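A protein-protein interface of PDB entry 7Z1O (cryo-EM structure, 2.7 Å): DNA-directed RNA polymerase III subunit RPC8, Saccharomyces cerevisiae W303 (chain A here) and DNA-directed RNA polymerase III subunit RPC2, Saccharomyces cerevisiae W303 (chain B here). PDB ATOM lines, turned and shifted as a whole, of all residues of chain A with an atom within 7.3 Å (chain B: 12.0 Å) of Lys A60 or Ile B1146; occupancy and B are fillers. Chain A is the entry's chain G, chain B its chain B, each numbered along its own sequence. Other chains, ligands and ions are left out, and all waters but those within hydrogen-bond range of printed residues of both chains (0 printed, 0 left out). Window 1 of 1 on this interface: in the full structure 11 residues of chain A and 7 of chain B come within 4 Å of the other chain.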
ATOM      1  N   ARG A  12     -22.492 -19.793  19.464  1.00  0.00           N
ATOM      2  CA  ARG A  12     -21.297 -19.036  19.811  1.00  0.00           C
ATOM      3  C   ARG A  12     -20.948 -19.329  21.265  1.00  0.00           C
ATOM      4  O   ARG A  12     -21.651 -18.889  22.180  1.00  0.00           O
ATOM      5  CB  ARG A  12     -21.520 -17.543  19.588  1.00  0.00           C
ATOM      6  CG  ARG A  12     -20.414 -16.662  20.131  1.00  0.00           C
ATOM      7  CD  ARG A  12     -20.710 -15.196  19.884  1.00  0.00           C
ATOM      8  NE  ARG A  12     -19.696 -14.328  20.467  1.00  0.00           N
ATOM      9  CZ  ARG A  12     -19.655 -13.974  21.744  1.00  0.00           C
ATOM     10  NH1 ARG A  12     -20.567 -14.392  22.606  1.00  0.00           N
ATOM     11  NH2 ARG A  12     -18.676 -13.180  22.167  1.00  0.00           N
ATOM     12  N   GLN A  58     -15.165 -22.842  14.475  1.00  0.00           N
ATOM     13  CA  GLN A  58     -14.483 -21.836  13.676  1.00  0.00           C
ATOM     14  C   GLN A  58     -14.434 -20.519  14.435  1.00  0.00           C
ATOM     15  O   GLN A  58     -15.356 -20.187  15.183  1.00  0.00           O
ATOM     16  CB  GLN A  58     -15.190 -21.647  12.336  1.00  0.00           C
ATOM     17  CG  GLN A  58     -15.644 -22.945  11.705  1.00  0.00           C
ATOM     18  CD  GLN A  58     -16.423 -22.728  10.431  1.00  0.00           C
ATOM     19  OE1 GLN A  58     -16.180 -21.773   9.696  1.00  0.00           O
ATOM     20  NE2 GLN A  58     -17.372 -23.616  10.160  1.00  0.00           N
ATOM     21  N   LEU A  59     -13.352 -19.773  14.241  1.00  0.00           N
ATOM     22  CA  LEU A  59     -13.110 -18.543  14.982  1.00  0.00           C
ATOM     23  C   LEU A  59     -13.110 -17.353  14.035  1.00  0.00           C
ATOM     24  O   LEU A  59     -12.404 -17.354  13.023  1.00  0.00           O
ATOM     25  CB  LEU A  59     -11.787 -18.602  15.749  1.00  0.00           C
ATOM     26  CG  LEU A  59     -11.755 -19.393  17.059  1.00  0.00           C
ATOM     27  CD1 LEU A  59     -11.803 -20.887  16.833  1.00  0.00           C
ATOM     28  CD2 LEU A  59     -10.546 -19.026  17.876  1.00  0.00           C
ATOM     29  N   LYS A  60     -13.901 -16.355  14.370  1.00  0.00           N
ATOM     30  CA  LYS A  60     -13.951 -15.094  13.649  1.00  0.00           C
ATOM     31  C   LYS A  60     -12.704 -14.268  13.962  1.00  0.00           C
ATOM     32  O   LYS A  60     -12.302 -14.175  15.125  1.00  0.00           O
ATOM     33  CB  LYS A  60     -15.204 -14.316  14.039  1.00  0.00           C
ATOM     34  CG  LYS A  60     -15.625 -13.247  13.058  1.00  0.00           C
ATOM     35  CD  LYS A  60     -17.055 -12.818  13.321  1.00  0.00           C
ATOM     36  CE  LYS A  60     -17.199 -12.202  14.699  1.00  0.00           C
ATOM     37  NZ  LYS A  60     -18.382 -11.304  14.780  1.00  0.00           N
ATOM     38  N   PRO A  61     -12.067 -13.676  12.951  1.00  0.00           N
ATOM     39  CA  PRO A  61     -10.907 -12.809  13.212  1.00  0.00           C
ATOM     40  C   PRO A  61     -11.334 -11.555  13.964  1.00  0.00           C
ATOM     41  O   PRO A  61     -12.071 -10.720  13.438  1.00  0.00           O
ATOM     42  CB  PRO A  61     -10.383 -12.482  11.809  1.00  0.00           C
ATOM     43  CG  PRO A  61     -11.535 -12.727  10.896  1.00  0.00           C
ATOM     44  CD  PRO A  61     -12.325 -13.840  11.511  1.00  0.00           C
ATOM     45  N   GLY A  62     -10.867 -11.433  15.204  1.00  0.00           N
ATOM     46  CA  GLY A  62     -11.245 -10.337  16.074  1.00  0.00           C
ATOM     47  C   GLY A  62     -12.064 -10.737  17.281  1.00  0.00           C
ATOM     48  O   GLY A  62     -12.430  -9.863  18.074  1.00  0.00           O
ATOM     49  N   ASP A  63     -12.365 -12.022  17.450  1.00  0.00           N
ATOM     50  CA  ASP A  63     -13.117 -12.497  18.600  1.00  0.00           C
ATOM     51  C   ASP A  63     -12.631 -13.890  18.969  1.00  0.00           C
ATOM     52  O   ASP A  63     -12.419 -14.731  18.091  1.00  0.00           O
ATOM     53  CB  ASP A  63     -14.623 -12.518  18.319  1.00  0.00           C
ATOM     54  CG  ASP A  63     -15.453 -12.488  19.587  1.00  0.00           C
ATOM     55  OD1 ASP A  63     -14.862 -12.394  20.683  1.00  0.00           O
ATOM     56  OD2 ASP A  63     -16.696 -12.560  19.489  1.00  0.00           O
ATOM     57  N   GLY A  64     -12.454 -14.125  20.268  1.00  0.00           N
ATOM     58  CA  GLY A  64     -11.991 -15.416  20.738  1.00  0.00           C
ATOM     59  C   GLY A  64     -13.064 -16.466  20.899  1.00  0.00           C
ATOM     60  O   GLY A  64     -12.737 -17.628  21.161  1.00  0.00           O
ATOM     61  N   SER A  65     -14.332 -16.088  20.760  1.00  0.00           N
ATOM     62  CA  SER A  65     -15.420 -17.045  20.885  1.00  0.00           C
ATOM     63  C   SER A  65     -15.403 -18.021  19.717  1.00  0.00           C
ATOM     64  O   SER A  65     -14.982 -17.689  18.606  1.00  0.00           O
ATOM     65  CB  SER A  65     -16.762 -16.317  20.947  1.00  0.00           C
ATOM     66  OG  SER A  65     -17.042 -15.659  19.725  1.00  0.00           O
ATOM     67  N   SER A  66     -15.865 -19.240  19.974  1.00  0.00           N
ATOM     68  CA  SER A  66     -15.850 -20.302  18.979  1.00  0.00           C
ATOM     69  C   SER A  66     -17.255 -20.511  18.435  1.00  0.00           C
ATOM     70  O   SER A  66     -18.203 -20.684  19.206  1.00  0.00           O
ATOM     71  CB  SER A  66     -15.310 -21.603  19.573  1.00  0.00           C
ATOM     72  OG  SER A  66     -16.344 -22.355  20.179  1.00  0.00           O
ATOM     73  N   TYR A  67     -17.386 -20.496  17.114  1.00  0.00           N
ATOM     74  CA  TYR A  67     -18.668 -20.688  16.452  1.00  0.00           C
ATOM     75  C   TYR A  67     -18.741 -22.117  15.936  1.00  0.00           C
ATOM     76  O   TYR A  67     -17.870 -22.553  15.176  1.00  0.00           O
ATOM     77  CB  TYR A  67     -18.855 -19.690  15.311  1.00  0.00           C
ATOM     78  CG  TYR A  67     -18.999 -18.254  15.762  1.00  0.00           C
ATOM     79  CD1 TYR A  67     -17.896 -17.516  16.163  1.00  0.00           C
ATOM     80  CD2 TYR A  67     -20.241 -17.637  15.782  1.00  0.00           C
ATOM     81  CE1 TYR A  67     -18.025 -16.208  16.572  1.00  0.00           C
ATOM     82  CE2 TYR A  67     -20.378 -16.328  16.189  1.00  0.00           C
ATOM     83  CZ  TYR A  67     -19.267 -15.619  16.583  1.00  0.00           C
ATOM     84  OH  TYR A  67     -19.397 -14.313  16.990  1.00  0.00           O
ATOM     85  N   SER B1076      -2.464  -8.386   9.132  1.00  0.00           N
ATOM     86  CA  SER B1076      -3.810  -7.976   8.750  1.00  0.00           C
ATOM     87  C   SER B1076      -4.585  -7.385   9.923  1.00  0.00           C
ATOM     88  O   SER B1076      -5.265  -6.363   9.769  1.00  0.00           O
ATOM     89  CB  SER B1076      -4.568  -9.163   8.159  1.00  0.00           C
ATOM     90  OG  SER B1076      -4.654 -10.225   9.090  1.00  0.00           O
ATOM     91  N   GLN B1077      -4.494  -8.016  11.097  1.00  0.00           N
ATOM     92  CA  GLN B1077      -5.254  -7.551  12.254  1.00  0.00           C
ATOM     93  C   GLN B1077      -4.763  -6.194  12.735  1.00  0.00           C
ATOM     94  O   GLN B1077      -5.564  -5.360  13.170  1.00  0.00           O
ATOM     95  CB  GLN B1077      -5.182  -8.576  13.382  1.00  0.00           C
ATOM     96  CG  GLN B1077      -5.873  -9.883  13.062  1.00  0.00           C
ATOM     97  CD  GLN B1077      -7.326  -9.690  12.694  1.00  0.00           C
ATOM     98  OE1 GLN B1077      -8.062  -8.985  13.382  1.00  0.00           O
ATOM     99  NE2 GLN B1077      -7.747 -10.316  11.603  1.00  0.00           N
ATOM    100  N   LEU B1080      -6.230  -3.653  10.376  1.00  0.00           N
ATOM    101  CA  LEU B1080      -7.651  -3.482  10.660  1.00  0.00           C
ATOM    102  C   LEU B1080      -7.875  -2.666  11.929  1.00  0.00           C
ATOM    103  O   LEU B1080      -8.778  -1.825  11.981  1.00  0.00           O
ATOM    104  CB  LEU B1080      -8.323  -4.849  10.773  1.00  0.00           C
ATOM    105  CG  LEU B1080      -9.822  -4.877  11.053  1.00  0.00           C
ATOM    106  CD1 LEU B1080     -10.601  -4.817   9.759  1.00  0.00           C
ATOM    107  CD2 LEU B1080     -10.189  -6.120  11.842  1.00  0.00           C
ATOM    108  N   MET B1084      -9.467   0.911  11.119  1.00  0.00           N
ATOM    109  CA  MET B1084     -10.905   0.864  11.363  1.00  0.00           C
ATOM    110  C   MET B1084     -11.254   1.043  12.835  1.00  0.00           C
ATOM    111  O   MET B1084     -12.073   1.907  13.160  1.00  0.00           O
ATOM    112  CB  MET B1084     -11.496  -0.438  10.804  1.00  0.00           C
ATOM    113  CG  MET B1084     -13.013  -0.509  10.876  1.00  0.00           C
ATOM    114  SD  MET B1084     -13.675  -2.169  10.655  1.00  0.00           S
ATOM    115  CE  MET B1084     -13.077  -2.993  12.122  1.00  0.00           C
ATOM    116  N   ILE B1085     -10.655   0.261  13.737  1.00  0.00           N
ATOM    117  CA  ILE B1085     -11.023   0.319  15.151  1.00  0.00           C
ATOM    118  C   ILE B1085     -10.644   1.661  15.765  1.00  0.00           C
ATOM    119  O   ILE B1085     -11.442   2.278  16.481  1.00  0.00           O
ATOM    120  CB  ILE B1085     -10.379  -0.849  15.920  1.00  0.00           C
ATOM    121  CG1 ILE B1085     -10.864  -2.192  15.374  1.00  0.00           C
ATOM    122  CG2 ILE B1085     -10.672  -0.742  17.408  1.00  0.00           C
ATOM    123  CD1 ILE B1085     -12.326  -2.452  15.642  1.00  0.00           C
ATOM    124  N   GLU B1091     -21.044   1.123  13.239  1.00  0.00           N
ATOM    125  CA  GLU B1091     -21.998   0.034  13.080  1.00  0.00           C
ATOM    126  C   GLU B1091     -23.159   0.504  12.214  1.00  0.00           C
ATOM    127  O   GLU B1091     -23.799   1.516  12.518  1.00  0.00           O
ATOM    128  CB  GLU B1091     -22.504  -0.449  14.438  1.00  0.00           C
ATOM    129  CG  GLU B1091     -21.441  -1.122  15.288  1.00  0.00           C
ATOM    130  CD  GLU B1091     -21.968  -1.573  16.635  1.00  0.00           C
ATOM    131  OE1 GLU B1091     -23.131  -1.251  16.958  1.00  0.00           O
ATOM    132  OE2 GLU B1091     -21.219  -2.250  17.371  1.00  0.00           O
ATOM    133  N   ASP B1096     -29.784  -7.074   2.743  1.00  0.00           N
ATOM    134  CA  ASP B1096     -29.227  -8.212   2.027  1.00  0.00           C
ATOM    135  C   ASP B1096     -29.789  -8.368   0.621  1.00  0.00           C
ATOM    136  O   ASP B1096     -29.204  -9.100  -0.185  1.00  0.00           O
ATOM    137  CB  ASP B1096     -29.474  -9.499   2.815  1.00  0.00           C
ATOM    138  CG  ASP B1096     -28.452 -10.573   2.512  1.00  0.00           C
ATOM    139  OD1 ASP B1096     -27.452 -10.269   1.830  1.00  0.00           O
ATOM    140  OD2 ASP B1096     -28.648 -11.723   2.957  1.00  0.00           O
ATOM    141  N   ILE B1117     -28.899  -6.484   8.203  1.00  0.00           N
ATOM    142  CA  ILE B1117     -27.773  -7.139   8.852  1.00  0.00           C
ATOM    143  C   ILE B1117     -26.886  -6.070   9.476  1.00  0.00           C
ATOM    144  O   ILE B1117     -26.547  -5.079   8.819  1.00  0.00           O
ATOM    145  CB  ILE B1117     -26.975  -8.002   7.856  1.00  0.00           C
ATOM    146  CG1 ILE B1117     -27.846  -9.153   7.357  1.00  0.00           C
ATOM    147  CG2 ILE B1117     -25.711  -8.541   8.498  1.00  0.00           C
ATOM    148  CD1 ILE B1117     -27.562  -9.561   5.944  1.00  0.00           C
ATOM    149  N   LYS B1118     -26.540  -6.261  10.749  1.00  0.00           N
ATOM    150  CA  LYS B1118     -25.599  -5.390  11.437  1.00  0.00           C
ATOM    151  C   LYS B1118     -24.189  -5.666  10.933  1.00  0.00           C
ATOM    152  O   LYS B1118     -23.752  -6.820  10.907  1.00  0.00           O
ATOM    153  CB  LYS B1118     -25.654  -5.636  12.945  1.00  0.00           C
ATOM    154  CG  LYS B1118     -26.966  -5.301  13.629  1.00  0.00           C
ATOM    155  CD  LYS B1118     -27.358  -3.856  13.442  1.00  0.00           C
ATOM    156  CE  LYS B1118     -28.758  -3.602  13.982  1.00  0.00           C
ATOM    157  NZ  LYS B1118     -29.800  -4.306  13.184  1.00  0.00           N
ATOM    158  N   MET B1119     -23.472  -4.614  10.540  1.00  0.00           N
ATOM    159  CA  MET B1119     -22.078  -4.768  10.150  1.00  0.00           C
ATOM    160  C   MET B1119     -21.272  -3.607  10.707  1.00  0.00           C
ATOM    161  O   MET B1119     -21.820  -2.610  11.175  1.00  0.00           O
ATOM    162  CB  MET B1119     -21.907  -4.852   8.631  1.00  0.00           C
ATOM    163  CG  MET B1119     -22.498  -6.093   8.001  1.00  0.00           C
ATOM    164  SD  MET B1119     -22.318  -6.065   6.222  1.00  0.00           S
ATOM    165  CE  MET B1119     -20.552  -6.308   6.117  1.00  0.00           C
ATOM    166  N   THR B1120     -19.951  -3.754  10.658  1.00  0.00           N
ATOM    167  CA  THR B1120     -19.023  -2.725  11.107  1.00  0.00           C
ATOM    168  C   THR B1120     -18.163  -2.300   9.928  1.00  0.00           C
ATOM    169  O   THR B1120     -17.443  -3.122   9.354  1.00  0.00           O
ATOM    170  CB  THR B1120     -18.148  -3.232  12.255  1.00  0.00           C
ATOM    171  OG1 THR B1120     -18.970  -3.527  13.391  1.00  0.00           O
ATOM    172  CG2 THR B1120     -17.119  -2.184  12.642  1.00  0.00           C
ATOM    173  N   ILE B1121     -18.243  -1.023   9.567  1.00  0.00           N
ATOM    174  CA  ILE B1121     -17.441  -0.475   8.476  1.00  0.00           C
ATOM    175  C   ILE B1121     -16.799   0.822   8.937  1.00  0.00           C
ATOM    176  O   ILE B1121     -17.246   1.447   9.908  1.00  0.00           O
ATOM    177  CB  ILE B1121     -18.279  -0.225   7.204  1.00  0.00           C
ATOM    178  CG1 ILE B1121     -19.496   0.645   7.515  1.00  0.00           C
ATOM    179  CG2 ILE B1121     -18.693  -1.537   6.557  1.00  0.00           C
ATOM    180  CD1 ILE B1121     -20.181   1.179   6.281  1.00  0.00           C
ATOM    181  N   ARG B1142     -22.798  -6.885  -1.545  1.00  0.00           N
ATOM    182  CA  ARG B1142     -23.252  -8.266  -1.543  1.00  0.00           C
ATOM    183  C   ARG B1142     -22.598  -8.987  -0.377  1.00  0.00           C
ATOM    184  O   ARG B1142     -21.373  -8.950  -0.228  1.00  0.00           O
ATOM    185  CB  ARG B1142     -22.919  -8.960  -2.865  1.00  0.00           C
ATOM    186  CG  ARG B1142     -23.555  -8.298  -4.070  1.00  0.00           C
ATOM    187  CD  ARG B1142     -25.052  -8.179  -3.880  1.00  0.00           C
ATOM    188  NE  ARG B1142     -25.700  -7.520  -5.006  1.00  0.00           N
ATOM    189  CZ  ARG B1142     -26.937  -7.047  -4.982  1.00  0.00           C
ATOM    190  NH1 ARG B1142     -27.686  -7.131  -3.897  1.00  0.00           N
ATOM    191  NH2 ARG B1142     -27.432  -6.473  -6.074  1.00  0.00           N
ATOM    192  N   LEU B1143     -23.411  -9.639   0.448  1.00  0.00           N
ATOM    193  CA  LEU B1143     -22.946 -10.220   1.694  1.00  0.00           C
ATOM    194  C   LEU B1143     -23.023 -11.740   1.653  1.00  0.00           C
ATOM    195  O   LEU B1143     -23.900 -12.322   1.010  1.00  0.00           O
ATOM    196  CB  LEU B1143     -23.758  -9.698   2.880  1.00  0.00           C
ATOM    197  CG  LEU B1143     -24.021  -8.194   2.907  1.00  0.00           C
ATOM    198  CD1 LEU B1143     -24.844  -7.835   4.123  1.00  0.00           C
ATOM    199  CD2 LEU B1143     -22.717  -7.423   2.896  1.00  0.00           C
ATOM    200  N   GLU B1144     -22.086 -12.375   2.353  1.00  0.00           N
ATOM    201  CA  GLU B1144     -22.046 -13.822   2.487  1.00  0.00           C
ATOM    202  C   GLU B1144     -21.641 -14.175   3.910  1.00  0.00           C
ATOM    203  O   GLU B1144     -21.056 -13.362   4.630  1.00  0.00           O
ATOM    204  CB  GLU B1144     -21.079 -14.461   1.484  1.00  0.00           C
ATOM    205  CG  GLU B1144     -19.615 -14.167   1.759  1.00  0.00           C
ATOM    206  CD  GLU B1144     -18.688 -14.928   0.833  1.00  0.00           C
ATOM    207  OE1 GLU B1144     -19.185 -15.751   0.036  1.00  0.00           O
ATOM    208  OE2 GLU B1144     -17.462 -14.705   0.904  1.00  0.00           O
ATOM    209  N   ASP B1145     -21.968 -15.400   4.311  1.00  0.00           N
ATOM    210  CA  ASP B1145     -21.642 -15.865   5.651  1.00  0.00           C
ATOM    211  C   ASP B1145     -20.137 -16.033   5.815  1.00  0.00           C
ATOM    212  O   ASP B1145     -19.436 -16.449   4.890  1.00  0.00           O
ATOM    213  CB  ASP B1145     -22.347 -17.189   5.937  1.00  0.00           C
ATOM    214  CG  ASP B1145     -23.848 -17.037   6.046  1.00  0.00           C
ATOM    215  OD1 ASP B1145     -24.308 -15.947   6.442  1.00  0.00           O
ATOM    216  OD2 ASP B1145     -24.570 -18.008   5.735  1.00  0.00           O
ATOM    217  N   ILE B1146     -19.643 -15.698   7.008  1.00  0.00           N
ATOM    218  CA  ILE B1146     -18.225 -15.877   7.303  1.00  0.00           C
ATOM    219  C   ILE B1146     -17.883 -17.358   7.395  1.00  0.00           C
ATOM    220  O   ILE B1146     -16.824 -17.796   6.930  1.00  0.00           O
ATOM    221  CB  ILE B1146     -17.853 -15.125   8.593  1.00  0.00           C
ATOM    222  CG1 ILE B1146     -18.244 -13.653   8.479  1.00  0.00           C
ATOM    223  CG2 ILE B1146     -16.366 -15.247   8.878  1.00  0.00           C
ATOM    224  CD1 ILE B1146     -17.902 -12.836   9.700  1.00  0.00           C
ATOM    225  N   PHE B1147     -18.774 -18.151   7.977  1.00  0.00           N
ATOM    226  CA  PHE B1147     -18.548 -19.573   8.188  1.00  0.00           C
ATOM    227  C   PHE B1147     -19.206 -20.365   7.069  1.00  0.00           C
ATOM    228  O   PHE B1147     -20.362 -20.108   6.716  1.00  0.00           O
ATOM    229  CB  PHE B1147     -19.089 -19.996   9.552  1.00  0.00           C
ATOM    230  CG  PHE B1147     -18.632 -19.109  10.669  1.00  0.00           C
ATOM    231  CD1 PHE B1147     -17.289 -19.013  10.984  1.00  0.00           C
ATOM    232  CD2 PHE B1147     -19.537 -18.349  11.384  1.00  0.00           C
ATOM    233  CE1 PHE B1147     -16.859 -18.190  11.999  1.00  0.00           C
ATOM    234  CE2 PHE B1147     -19.112 -17.523  12.402  1.00  0.00           C
ATOM    235  CZ  PHE B1147     -17.770 -17.444  12.708  1.00  0.00           C
ATOM    236  N   GLN B1148     -18.457 -21.320   6.509  1.00  0.00           N
ATOM    237  CA  GLN B1148     -18.902 -22.020   5.307  1.00  0.00           C
ATOM    238  C   GLN B1148     -20.148 -22.856   5.571  1.00  0.00           C
ATOM    239  O   GLN B1148     -21.041 -22.931   4.718  1.00  0.00           O
ATOM    240  CB  GLN B1148     -17.771 -22.895   4.766  1.00  0.00           C
ATOM    241  CG  GLN B1148     -16.595 -22.106   4.212  1.00  0.00           C
ATOM    242  CD  GLN B1148     -15.535 -22.995   3.591  1.00  0.00           C
ATOM    243  OE1 GLN B1148     -15.573 -24.217   3.734  1.00  0.00           O
ATOM    244  NE2 GLN B1148     -14.582 -22.385   2.898  1.00  0.00           N
ATOM    245  N   GLN B1149     -20.216 -23.495   6.740  1.00  0.00           N
ATOM    246  CA  GLN B1149     -21.361 -24.306   7.167  1.00  0.00           C
ATOM    247  C   GLN B1149     -21.693 -25.427   6.184  1.00  0.00           C
ATOM    248  O   GLN B1149     -20.922 -26.371   6.021  1.00  0.00           O
ATOM    249  CB  GLN B1149     -22.592 -23.421   7.391  1.00  0.00           C
ATOM    250  CG  GLN B1149     -23.741 -24.114   8.098  1.00  0.00           C
ATOM    251  CD  GLN B1149     -24.844 -23.152   8.489  1.00  0.00           C
ATOM    252  OE1 GLN B1149     -24.849 -21.994   8.074  1.00  0.00           O
ATOM    253  NE2 GLN B1149     -25.785 -23.626   9.298  1.00  0.00           N
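The guanidinium group (NE) of Arg A12 lies close to the side-chain hydroxyl (OH) of Tyr A67. The backbone NH (N) of Gln A58 lies within hydrogen-bond range of the backbone carbonyl oxygen (O) of Tyr A67 (2.8 Å).
Among the printed residues, merely in contact across the chains: Gln A58 with Phe B1147, Gln A58 with Gln B1148, Lys A60 with Ile B1146, Pro A61 with Gln B1077 and Tyr A67 with Phe B1147.
Pro A61 touches just one residue of chain B: Gln B1077 (3.4 Å). No residue of chain B comes within 4 Å of Gly A64. No residue of chain B comes within 4 Å of Ser A65. Ser B1076 touches none of the printed residues of chain A. Printed residues of chain A within 4 Å of Gln B1077: Pro A61. Of chain A, only Lys A60 comes within 4 Å of Ile B1146. Of the printed residues of chain A, Phe B1147 touches Gln A58 (3.2 Å) and Tyr A67 (3.4 Å). Of the printed residues of chain A, Gln B1148 touches Gln A58 (3.9 Å). The nearest printed residue of chain A that does not touch Phe B1147 is Lys A60 (4.2 Å).
Hydrophobic or aromatic side chains of chain B that line the printed part of chain A: Ile B1146 and Phe B1147. Among the printed residues, no Asp or Glu carboxylate lies within 4 Å of a Lys or Arg side-chain nitrogen of the other chain.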
